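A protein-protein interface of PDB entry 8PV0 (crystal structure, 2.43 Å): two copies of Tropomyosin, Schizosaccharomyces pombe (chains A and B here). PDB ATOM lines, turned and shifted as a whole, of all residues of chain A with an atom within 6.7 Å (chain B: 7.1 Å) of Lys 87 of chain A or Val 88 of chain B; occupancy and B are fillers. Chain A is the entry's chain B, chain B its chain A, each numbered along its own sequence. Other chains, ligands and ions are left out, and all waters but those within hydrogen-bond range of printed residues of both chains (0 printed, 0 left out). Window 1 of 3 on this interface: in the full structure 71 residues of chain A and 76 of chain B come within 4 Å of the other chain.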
ATOM      1  N   GLU A  82       4.673  20.491  -1.324  1.00  0.00           N
ATOM      2  CA  GLU A  82       5.436  19.867  -2.403  1.00  0.00           C
ATOM      3  C   GLU A  82       6.725  19.242  -1.881  1.00  0.00           C
ATOM      4  O   GLU A  82       7.108  18.140  -2.300  1.00  0.00           O
ATOM      5  CB  GLU A  82       5.734  20.897  -3.491  1.00  0.00           C
ATOM      6  CG  GLU A  82       4.495  21.369  -4.232  1.00  0.00           C
ATOM      7  CD  GLU A  82       4.782  22.502  -5.193  1.00  0.00           C
ATOM      8  OE1 GLU A  82       5.821  23.175  -5.032  1.00  0.00           O
ATOM      9  OE2 GLU A  82       3.967  22.720  -6.113  1.00  0.00           O
ATOM     10  N   GLN A  83       7.410  19.933  -0.964  1.00  0.00           N
ATOM     11  CA  GLN A  83       8.621  19.375  -0.367  1.00  0.00           C
ATOM     12  C   GLN A  83       8.319  18.092   0.395  1.00  0.00           C
ATOM     13  O   GLN A  83       9.078  17.120   0.313  1.00  0.00           O
ATOM     14  CB  GLN A  83       9.275  20.398   0.562  1.00  0.00           C
ATOM     15  CG  GLN A  83       9.885  21.589  -0.145  1.00  0.00           C
ATOM     16  CD  GLN A  83      10.535  22.555   0.820  1.00  0.00           C
ATOM     17  OE1 GLN A  83      11.511  22.218   1.492  1.00  0.00           O
ATOM     18  NE2 GLN A  83       9.994  23.765   0.902  1.00  0.00           N
ATOM     19  N   LEU A  84       7.214  18.071   1.144  1.00  0.00           N
ATOM     20  CA  LEU A  84       6.855  16.869   1.890  1.00  0.00           C
ATOM     21  C   LEU A  84       6.505  15.718   0.953  1.00  0.00           C
ATOM     22  O   LEU A  84       6.837  14.560   1.234  1.00  0.00           O
ATOM     23  CB  LEU A  84       5.699  17.170   2.841  1.00  0.00           C
ATOM     24  CG  LEU A  84       6.078  18.066   4.019  1.00  0.00           C
ATOM     25  CD1 LEU A  84       4.850  18.461   4.812  1.00  0.00           C
ATOM     26  CD2 LEU A  84       7.084  17.358   4.906  1.00  0.00           C
ATOM     27  N   SER A  85       5.840  16.015  -0.166  1.00  0.00           N
ATOM     28  CA  SER A  85       5.560  14.970  -1.148  1.00  0.00           C
ATOM     29  C   SER A  85       6.852  14.401  -1.728  1.00  0.00           C
ATOM     30  O   SER A  85       7.004  13.175  -1.859  1.00  0.00           O
ATOM     31  CB  SER A  85       4.665  15.522  -2.257  1.00  0.00           C
ATOM     32  OG  SER A  85       4.351  14.519  -3.206  1.00  0.00           O
ATOM     33  N   ARG A  86       7.797  15.278  -2.077  1.00  0.00           N
ATOM     34  CA  ARG A  86       9.087  14.804  -2.571  1.00  0.00           C
ATOM     35  C   ARG A  86       9.807  13.969  -1.517  1.00  0.00           C
ATOM     36  O   ARG A  86      10.462  12.973  -1.844  1.00  0.00           O
ATOM     37  CB  ARG A  86       9.953  15.986  -3.011  1.00  0.00           C
ATOM     38  CG  ARG A  86       9.538  16.586  -4.347  1.00  0.00           C
ATOM     39  CD  ARG A  86      10.592  17.545  -4.885  1.00  0.00           C
ATOM     40  NE  ARG A  86      10.764  18.715  -4.033  1.00  0.00           N
ATOM     41  CZ  ARG A  86      10.114  19.861  -4.192  1.00  0.00           C
ATOM     42  NH1 ARG A  86       9.235  20.029  -5.166  1.00  0.00           N
ATOM     43  NH2 ARG A  86      10.354  20.864  -3.353  1.00  0.00           N
ATOM     44  N   LYS A  87       9.683  14.350  -0.243  1.00  0.00           N
ATOM     45  CA  LYS A  87      10.329  13.586   0.819  1.00  0.00           C
ATOM     46  C   LYS A  87       9.694  12.208   0.973  1.00  0.00           C
ATOM     47  O   LYS A  87      10.394  11.222   1.229  1.00  0.00           O
ATOM     48  CB  LYS A  87      10.265  14.359   2.136  1.00  0.00           C
ATOM     49  CG  LYS A  87      11.091  13.744   3.252  1.00  0.00           C
ATOM     50  CD  LYS A  87      11.128  14.653   4.469  1.00  0.00           C
ATOM     51  CE  LYS A  87      12.015  14.082   5.562  1.00  0.00           C
ATOM     52  NZ  LYS A  87      12.077  14.982   6.747  1.00  0.00           N
ATOM     53  N   VAL A  88       8.370  12.124   0.822  1.00  0.00           N
ATOM     54  CA  VAL A  88       7.693  10.827   0.848  1.00  0.00           C
ATOM     55  C   VAL A  88       8.211   9.940  -0.277  1.00  0.00           C
ATOM     56  O   VAL A  88       8.512   8.754  -0.076  1.00  0.00           O
ATOM     57  CB  VAL A  88       6.167  11.014   0.760  1.00  0.00           C
ATOM     58  CG1 VAL A  88       5.482   9.682   0.502  1.00  0.00           C
ATOM     59  CG2 VAL A  88       5.633  11.641   2.033  1.00  0.00           C
ATOM     60  N   GLU A  89       8.314  10.504  -1.485  1.00  0.00           N
ATOM     61  CA  GLU A  89       8.836   9.735  -2.614  1.00  0.00           C
ATOM     62  C   GLU A  89      10.259   9.255  -2.346  1.00  0.00           C
ATOM     63  O   GLU A  89      10.603   8.098  -2.632  1.00  0.00           O
ATOM     64  CB  GLU A  89       8.786  10.575  -3.891  1.00  0.00           C
ATOM     65  CG  GLU A  89       7.390  11.041  -4.280  1.00  0.00           C
ATOM     66  CD  GLU A  89       6.488   9.901  -4.716  1.00  0.00           C
ATOM     67  OE1 GLU A  89       6.967   9.006  -5.446  1.00  0.00           O
ATOM     68  OE2 GLU A  89       5.301   9.898  -4.327  1.00  0.00           O
ATOM     69  N   LEU A  90      11.098  10.134  -1.792  1.00  0.00           N
ATOM     70  CA  LEU A  90      12.476   9.768  -1.484  1.00  0.00           C
ATOM     71  C   LEU A  90      12.536   8.640  -0.461  1.00  0.00           C
ATOM     72  O   LEU A  90      13.333   7.704  -0.602  1.00  0.00           O
ATOM     73  CB  LEU A  90      13.237  10.992  -0.975  1.00  0.00           C
ATOM     74  CG  LEU A  90      14.617  10.750  -0.359  1.00  0.00           C
ATOM     75  CD1 LEU A  90      15.596  10.237  -1.406  1.00  0.00           C
ATOM     76  CD2 LEU A  90      15.137  12.018   0.299  1.00  0.00           C
ATOM     77  N   LEU A  91      11.700   8.712   0.576  1.00  0.00           N
ATOM     78  CA  LEU A  91      11.696   7.669   1.597  1.00  0.00           C
ATOM     79  C   LEU A  91      11.243   6.332   1.022  1.00  0.00           C
ATOM     80  O   LEU A  91      11.804   5.282   1.363  1.00  0.00           O
ATOM     81  CB  LEU A  91      10.804   8.084   2.766  1.00  0.00           C
ATOM     82  CG  LEU A  91      11.337   9.226   3.632  1.00  0.00           C
ATOM     83  CD1 LEU A  91      10.308   9.649   4.667  1.00  0.00           C
ATOM     84  CD2 LEU A  91      12.634   8.809   4.303  1.00  0.00           C
ATOM     85  N   GLU A  92      10.235   6.346   0.147  1.00  0.00           N
ATOM     86  CA  GLU A  92       9.785   5.094  -0.458  1.00  0.00           C
ATOM     87  C   GLU A  92      10.866   4.494  -1.354  1.00  0.00           C
ATOM     88  O   GLU A  92      11.073   3.269  -1.358  1.00  0.00           O
ATOM     89  CB  GLU A  92       8.490   5.327  -1.236  1.00  0.00           C
ATOM     90  CG  GLU A  92       7.294   5.647  -0.346  1.00  0.00           C
ATOM     91  CD  GLU A  92       6.050   6.001  -1.134  1.00  0.00           C
ATOM     92  OE1 GLU A  92       6.183   6.390  -2.313  1.00  0.00           O
ATOM     93  OE2 GLU A  92       4.939   5.889  -0.574  1.00  0.00           O
ATOM     94  N   GLU A  94      14.082   4.903  -0.942  1.00  0.00           N
ATOM     95  CA  GLU A  94      15.075   4.363  -0.017  1.00  0.00           C
ATOM     96  C   GLU A  94      14.640   3.012   0.532  1.00  0.00           C
ATOM     97  O   GLU A  94      15.461   2.098   0.680  1.00  0.00           O
ATOM     98  CB  GLU A  94      15.323   5.345   1.127  1.00  0.00           C
ATOM     99  CG  GLU A  94      16.247   6.495   0.779  1.00  0.00           C
ATOM    100  CD  GLU A  94      16.405   7.477   1.924  1.00  0.00           C
ATOM    101  OE1 GLU A  94      15.392   7.783   2.589  1.00  0.00           O
ATOM    102  OE2 GLU A  94      17.540   7.938   2.165  1.00  0.00           O
ATOM    103  N   GLU B  82       0.043  18.206   6.455  1.00  0.00           N
ATOM    104  CA  GLU B  82      -0.069  17.418   7.682  1.00  0.00           C
ATOM    105  C   GLU B  82      -0.097  15.922   7.372  1.00  0.00           C
ATOM    106  O   GLU B  82       0.599  15.117   8.016  1.00  0.00           O
ATOM    107  CB  GLU B  82      -1.321  17.831   8.456  1.00  0.00           C
ATOM    108  CG  GLU B  82      -1.331  19.283   8.888  1.00  0.00           C
ATOM    109  CD  GLU B  82      -2.674  19.708   9.443  1.00  0.00           C
ATOM    110  OE1 GLU B  82      -3.612  18.881   9.432  1.00  0.00           O
ATOM    111  OE2 GLU B  82      -2.792  20.868   9.890  1.00  0.00           O
ATOM    112  N   GLN B  83      -0.908  15.533   6.384  1.00  0.00           N
ATOM    113  CA  GLN B  83      -0.983  14.121   6.013  1.00  0.00           C
ATOM    114  C   GLN B  83       0.371  13.610   5.533  1.00  0.00           C
ATOM    115  O   GLN B  83       0.816  12.517   5.920  1.00  0.00           O
ATOM    116  CB  GLN B  83      -2.052  13.920   4.940  1.00  0.00           C
ATOM    117  CG  GLN B  83      -3.443  14.331   5.379  1.00  0.00           C
ATOM    118  CD  GLN B  83      -4.449  14.258   4.250  1.00  0.00           C
ATOM    119  OE1 GLN B  83      -4.091  14.016   3.098  1.00  0.00           O
ATOM    120  NE2 GLN B  83      -5.718  14.470   4.577  1.00  0.00           N
ATOM    121  N   LEU B  84       1.051  14.400   4.697  1.00  0.00           N
ATOM    122  CA  LEU B  84       2.354  13.986   4.196  1.00  0.00           C
ATOM    123  C   LEU B  84       3.384  13.882   5.315  1.00  0.00           C
ATOM    124  O   LEU B  84       4.275  13.031   5.253  1.00  0.00           O
ATOM    125  CB  LEU B  84       2.829  14.956   3.116  1.00  0.00           C
ATOM    126  CG  LEU B  84       1.983  14.981   1.843  1.00  0.00           C
ATOM    127  CD1 LEU B  84       2.459  16.077   0.906  1.00  0.00           C
ATOM    128  CD2 LEU B  84       2.012  13.627   1.151  1.00  0.00           C
ATOM    129  N   SER B  85       3.278  14.723   6.346  1.00  0.00           N
ATOM    130  CA  SER B  85       4.204  14.624   7.471  1.00  0.00           C
ATOM    131  C   SER B  85       3.996  13.328   8.242  1.00  0.00           C
ATOM    132  O   SER B  85       4.970  12.660   8.625  1.00  0.00           O
ATOM    133  CB  SER B  85       4.034  15.824   8.400  1.00  0.00           C
ATOM    134  OG  SER B  85       4.146  17.038   7.680  1.00  0.00           O
ATOM    135  N   ARG B  86       2.736  12.967   8.500  1.00  0.00           N
ATOM    136  CA  ARG B  86       2.482  11.681   9.145  1.00  0.00           C
ATOM    137  C   ARG B  86       3.038  10.532   8.310  1.00  0.00           C
ATOM    138  O   ARG B  86       3.652   9.593   8.846  1.00  0.00           O
ATOM    139  CB  ARG B  86       0.988  11.488   9.391  1.00  0.00           C
ATOM    140  CG  ARG B  86       0.418  12.386  10.469  1.00  0.00           C
ATOM    141  CD  ARG B  86      -0.901  11.839  10.981  1.00  0.00           C
ATOM    142  NE  ARG B  86      -1.764  11.385   9.899  1.00  0.00           N
ATOM    143  CZ  ARG B  86      -2.628  12.156   9.252  1.00  0.00           C
ATOM    144  NH1 ARG B  86      -2.760  13.440   9.541  1.00  0.00           N
ATOM    145  NH2 ARG B  86      -3.378  11.624   8.291  1.00  0.00           N
ATOM    146  N   LYS B  87       2.838  10.597   6.990  1.00  0.00           N
ATOM    147  CA  LYS B  87       3.390   9.573   6.107  1.00  0.00           C
ATOM    148  C   LYS B  87       4.911   9.521   6.205  1.00  0.00           C
ATOM    149  O   LYS B  87       5.506   8.434   6.214  1.00  0.00           O
ATOM    150  CB  LYS B  87       2.951   9.835   4.666  1.00  0.00           C
ATOM    151  CG  LYS B  87       3.329   8.737   3.681  1.00  0.00           C
ATOM    152  CD  LYS B  87       2.568   7.449   3.969  1.00  0.00           C
ATOM    153  CE  LYS B  87       2.843   6.387   2.913  1.00  0.00           C
ATOM    154  NZ  LYS B  87       2.060   5.145   3.171  1.00  0.00           N
ATOM    155  N   VAL B  88       5.555  10.688   6.284  1.00  0.00           N
ATOM    156  CA  VAL B  88       7.011  10.746   6.382  1.00  0.00           C
ATOM    157  C   VAL B  88       7.484  10.051   7.653  1.00  0.00           C
ATOM    158  O   VAL B  88       8.445   9.273   7.635  1.00  0.00           O
ATOM    159  CB  VAL B  88       7.494  12.207   6.328  1.00  0.00           C
ATOM    160  CG1 VAL B  88       8.885  12.335   6.931  1.00  0.00           C
ATOM    161  CG2 VAL B  88       7.495  12.710   4.898  1.00  0.00           C
ATOM    162  N   GLU B  89       6.812  10.323   8.774  1.00  0.00           N
ATOM    163  CA  GLU B  89       7.221   9.704  10.034  1.00  0.00           C
ATOM    164  C   GLU B  89       7.072   8.186   9.983  1.00  0.00           C
ATOM    165  O   GLU B  89       7.964   7.447  10.432  1.00  0.00           O
ATOM    166  CB  GLU B  89       6.416  10.287  11.197  1.00  0.00           C
ATOM    167  CG  GLU B  89       6.632   9.580  12.535  1.00  0.00           C
ATOM    168  CD  GLU B  89       8.070   9.651  13.043  1.00  0.00           C
ATOM    169  OE1 GLU B  89       8.841  10.523  12.587  1.00  0.00           O
ATOM    170  OE2 GLU B  89       8.428   8.826  13.913  1.00  0.00           O
ATOM    171  N   LEU B  90       5.949   7.702   9.441  1.00  0.00           N
ATOM    172  CA  LEU B  90       5.753   6.256   9.327  1.00  0.00           C
ATOM    173  C   LEU B  90       6.836   5.618   8.459  1.00  0.00           C
ATOM    174  O   LEU B  90       7.410   4.576   8.817  1.00  0.00           O
ATOM    175  CB  LEU B  90       4.360   5.957   8.768  1.00  0.00           C
ATOM    176  CG  LEU B  90       3.244   5.643   9.770  1.00  0.00           C
ATOM    177  CD1 LEU B  90       3.524   4.345  10.518  1.00  0.00           C
ATOM    178  CD2 LEU B  90       3.059   6.791  10.746  1.00  0.00           C
ATOM    179  N   LEU B  91       7.134   6.236   7.312  1.00  0.00           N
ATOM    180  CA  LEU B  91       8.155   5.687   6.426  1.00  0.00           C
ATOM    181  C   LEU B  91       9.528   5.706   7.088  1.00  0.00           C
ATOM    182  O   LEU B  91      10.327   4.785   6.893  1.00  0.00           O
ATOM    183  CB  LEU B  91       8.181   6.459   5.108  1.00  0.00           C
ATOM    184  CG  LEU B  91       6.937   6.328   4.228  1.00  0.00           C
ATOM    185  CD1 LEU B  91       7.058   7.228   3.009  1.00  0.00           C
ATOM    186  CD2 LEU B  91       6.727   4.883   3.809  1.00  0.00           C
ATOM    187  N   GLU B  92       9.816   6.735   7.888  1.00  0.00           N
ATOM    188  CA  GLU B  92      11.110   6.795   8.563  1.00  0.00           C
ATOM    189  C   GLU B  92      11.248   5.689   9.602  1.00  0.00           C
ATOM    190  O   GLU B  92      12.318   5.077   9.729  1.00  0.00           O
ATOM    191  CB  GLU B  92      11.304   8.160   9.215  1.00  0.00           C
ATOM    192  CG  GLU B  92      11.597   9.283   8.243  1.00  0.00           C
ATOM    193  CD  GLU B  92      11.817  10.605   8.949  1.00  0.00           C
ATOM    194  OE1 GLU B  92      11.725  10.636  10.196  1.00  0.00           O
ATOM    195  OE2 GLU B  92      12.083  11.611   8.259  1.00  0.00           O
ATOM    196  N   GLU B  93      10.184   5.425  10.363  1.00  0.00           N
ATOM    197  CA  GLU B  93      10.235   4.328  11.327  1.00  0.00           C
ATOM    198  C   GLU B  93      10.442   2.993  10.617  1.00  0.00           C
ATOM    199  O   GLU B  93      11.282   2.176  11.029  1.00  0.00           O
ATOM    200  CB  GLU B  93       8.959   4.308  12.170  1.00  0.00           C
ATOM    201  CG  GLU B  93       8.784   5.537  13.047  1.00  0.00           C
ATOM    202  CD  GLU B  93       7.403   5.622  13.671  1.00  0.00           C
ATOM    203  OE1 GLU B  93       6.532   4.803  13.310  1.00  0.00           O
ATOM    204  OE2 GLU B  93       7.186   6.510  14.524  1.00  0.00           O
ATOM    205  N   GLU B  94       9.685   2.760   9.538  1.00  0.00           N
ATOM    206  CA  GLU B  94       9.852   1.525   8.774  1.00  0.00           C
ATOM    207  C   GLU B  94      11.271   1.397   8.232  1.00  0.00           C
ATOM    208  O   GLU B  94      11.864   0.310   8.265  1.00  0.00           O
ATOM    209  CB  GLU B  94       8.834   1.478   7.633  1.00  0.00           C
ATOM    210  CG  GLU B  94       8.922   0.231   6.765  1.00  0.00           C
ATOM    211  CD  GLU B  94       7.908   0.231   5.631  1.00  0.00           C
ATOM    212  OE1 GLU B  94       7.158   1.223   5.498  1.00  0.00           O
ATOM    213  OE2 GLU B  94       7.861  -0.759   4.872  1.00  0.00           O
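Among the printed residues, merely in contact across the chains: Leu 84 of chain A with Ser 85 of chain B, Leu 91 of chain A with Val 88 of chain B, Ser 85 of chain A with Leu 84 of chain B, Val 88 of chain A with Val 88 of chain B, Leu 84 of chain A with Leu 84 of chain B, Glu 92 of chain A with Leu 91 of chain B, Val 88 of chain A with Leu 91 of chain B, Val 88 of chain A with Leu 84 of chain B, Leu 91 of chain A with Glu 92 of chain B, Lys 87 of chain A with Val 88 of chain B, Leu 91 of chain A with Leu 91 of chain B and Val 88 of chain A with Lys 87 of chain B.
Glu 82 of chain A touches none of the printed residues of chain B. Arg 86 of chain A touches none of the printed residues of chain B. Lys 87 of chain A touches just these residues of chain B: Val 88 (3.8 Å) and Glu 92 (3.7 Å). Printed residues of chain B within 4 Å of Val 88 of chain A: Leu 84 (3.8 Å), Lys 87 (3.95 Å), Val 88 (3.6 Å) and Leu 91 (3.7 Å). Printed residues of chain A within 4 Å of Lys 87 of chain B: Val 88. Val 88 of chain B touches just these residues of chain A: Lys 87, Val 88 and Leu 91. Of the printed residues of chain A, Glu 92 of chain B touches Lys 87 and Leu 91. The nearest residue of chain B that does not touch Lys 87 of chain A is Leu 91 of chain B (5.5 Å). The nearest residue of chain A that does not touch Val 88 of chain B is Leu 84 of chain A (4.2 Å). The nearest printed residue of chain B that does not touch Leu 84 of chain A is Val 88 of chain B (4.2 Å).
Lys 87 of chain A touches Val 88 of chain B, and with the chains exchanged Val 88 of chain A touches Lys 87 of chain B. Lys 87 of chain A touches Glu 92 of chain B, but with the chains exchanged Glu 92 of chain A does not touch Lys 87 of chain B (4.1 Å). Val 88 of chain A touches Leu 91 of chain B, and with the chains exchanged Leu 91 of chain A touches Val 88 of chain B. Leu 91 of chain A touches its own counterpart, Leu 91 of chain B.
OE2 of Glu 92 of chain B is in salt-bridge range of NZ of Lys 87 of chain A (3.7 Å).
Of the 13 printed residues of chain B, 6 touch a printed residue of chain A. Hydrophobic or aromatic side chains of chain B that line the printed part of chain A: Leu 84, Val 88 and Leu 91. Hydrophobic or aromatic side chains of chain A within 4 Å of the printed part of chain B: Leu 84, Val 88 and Leu 91.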
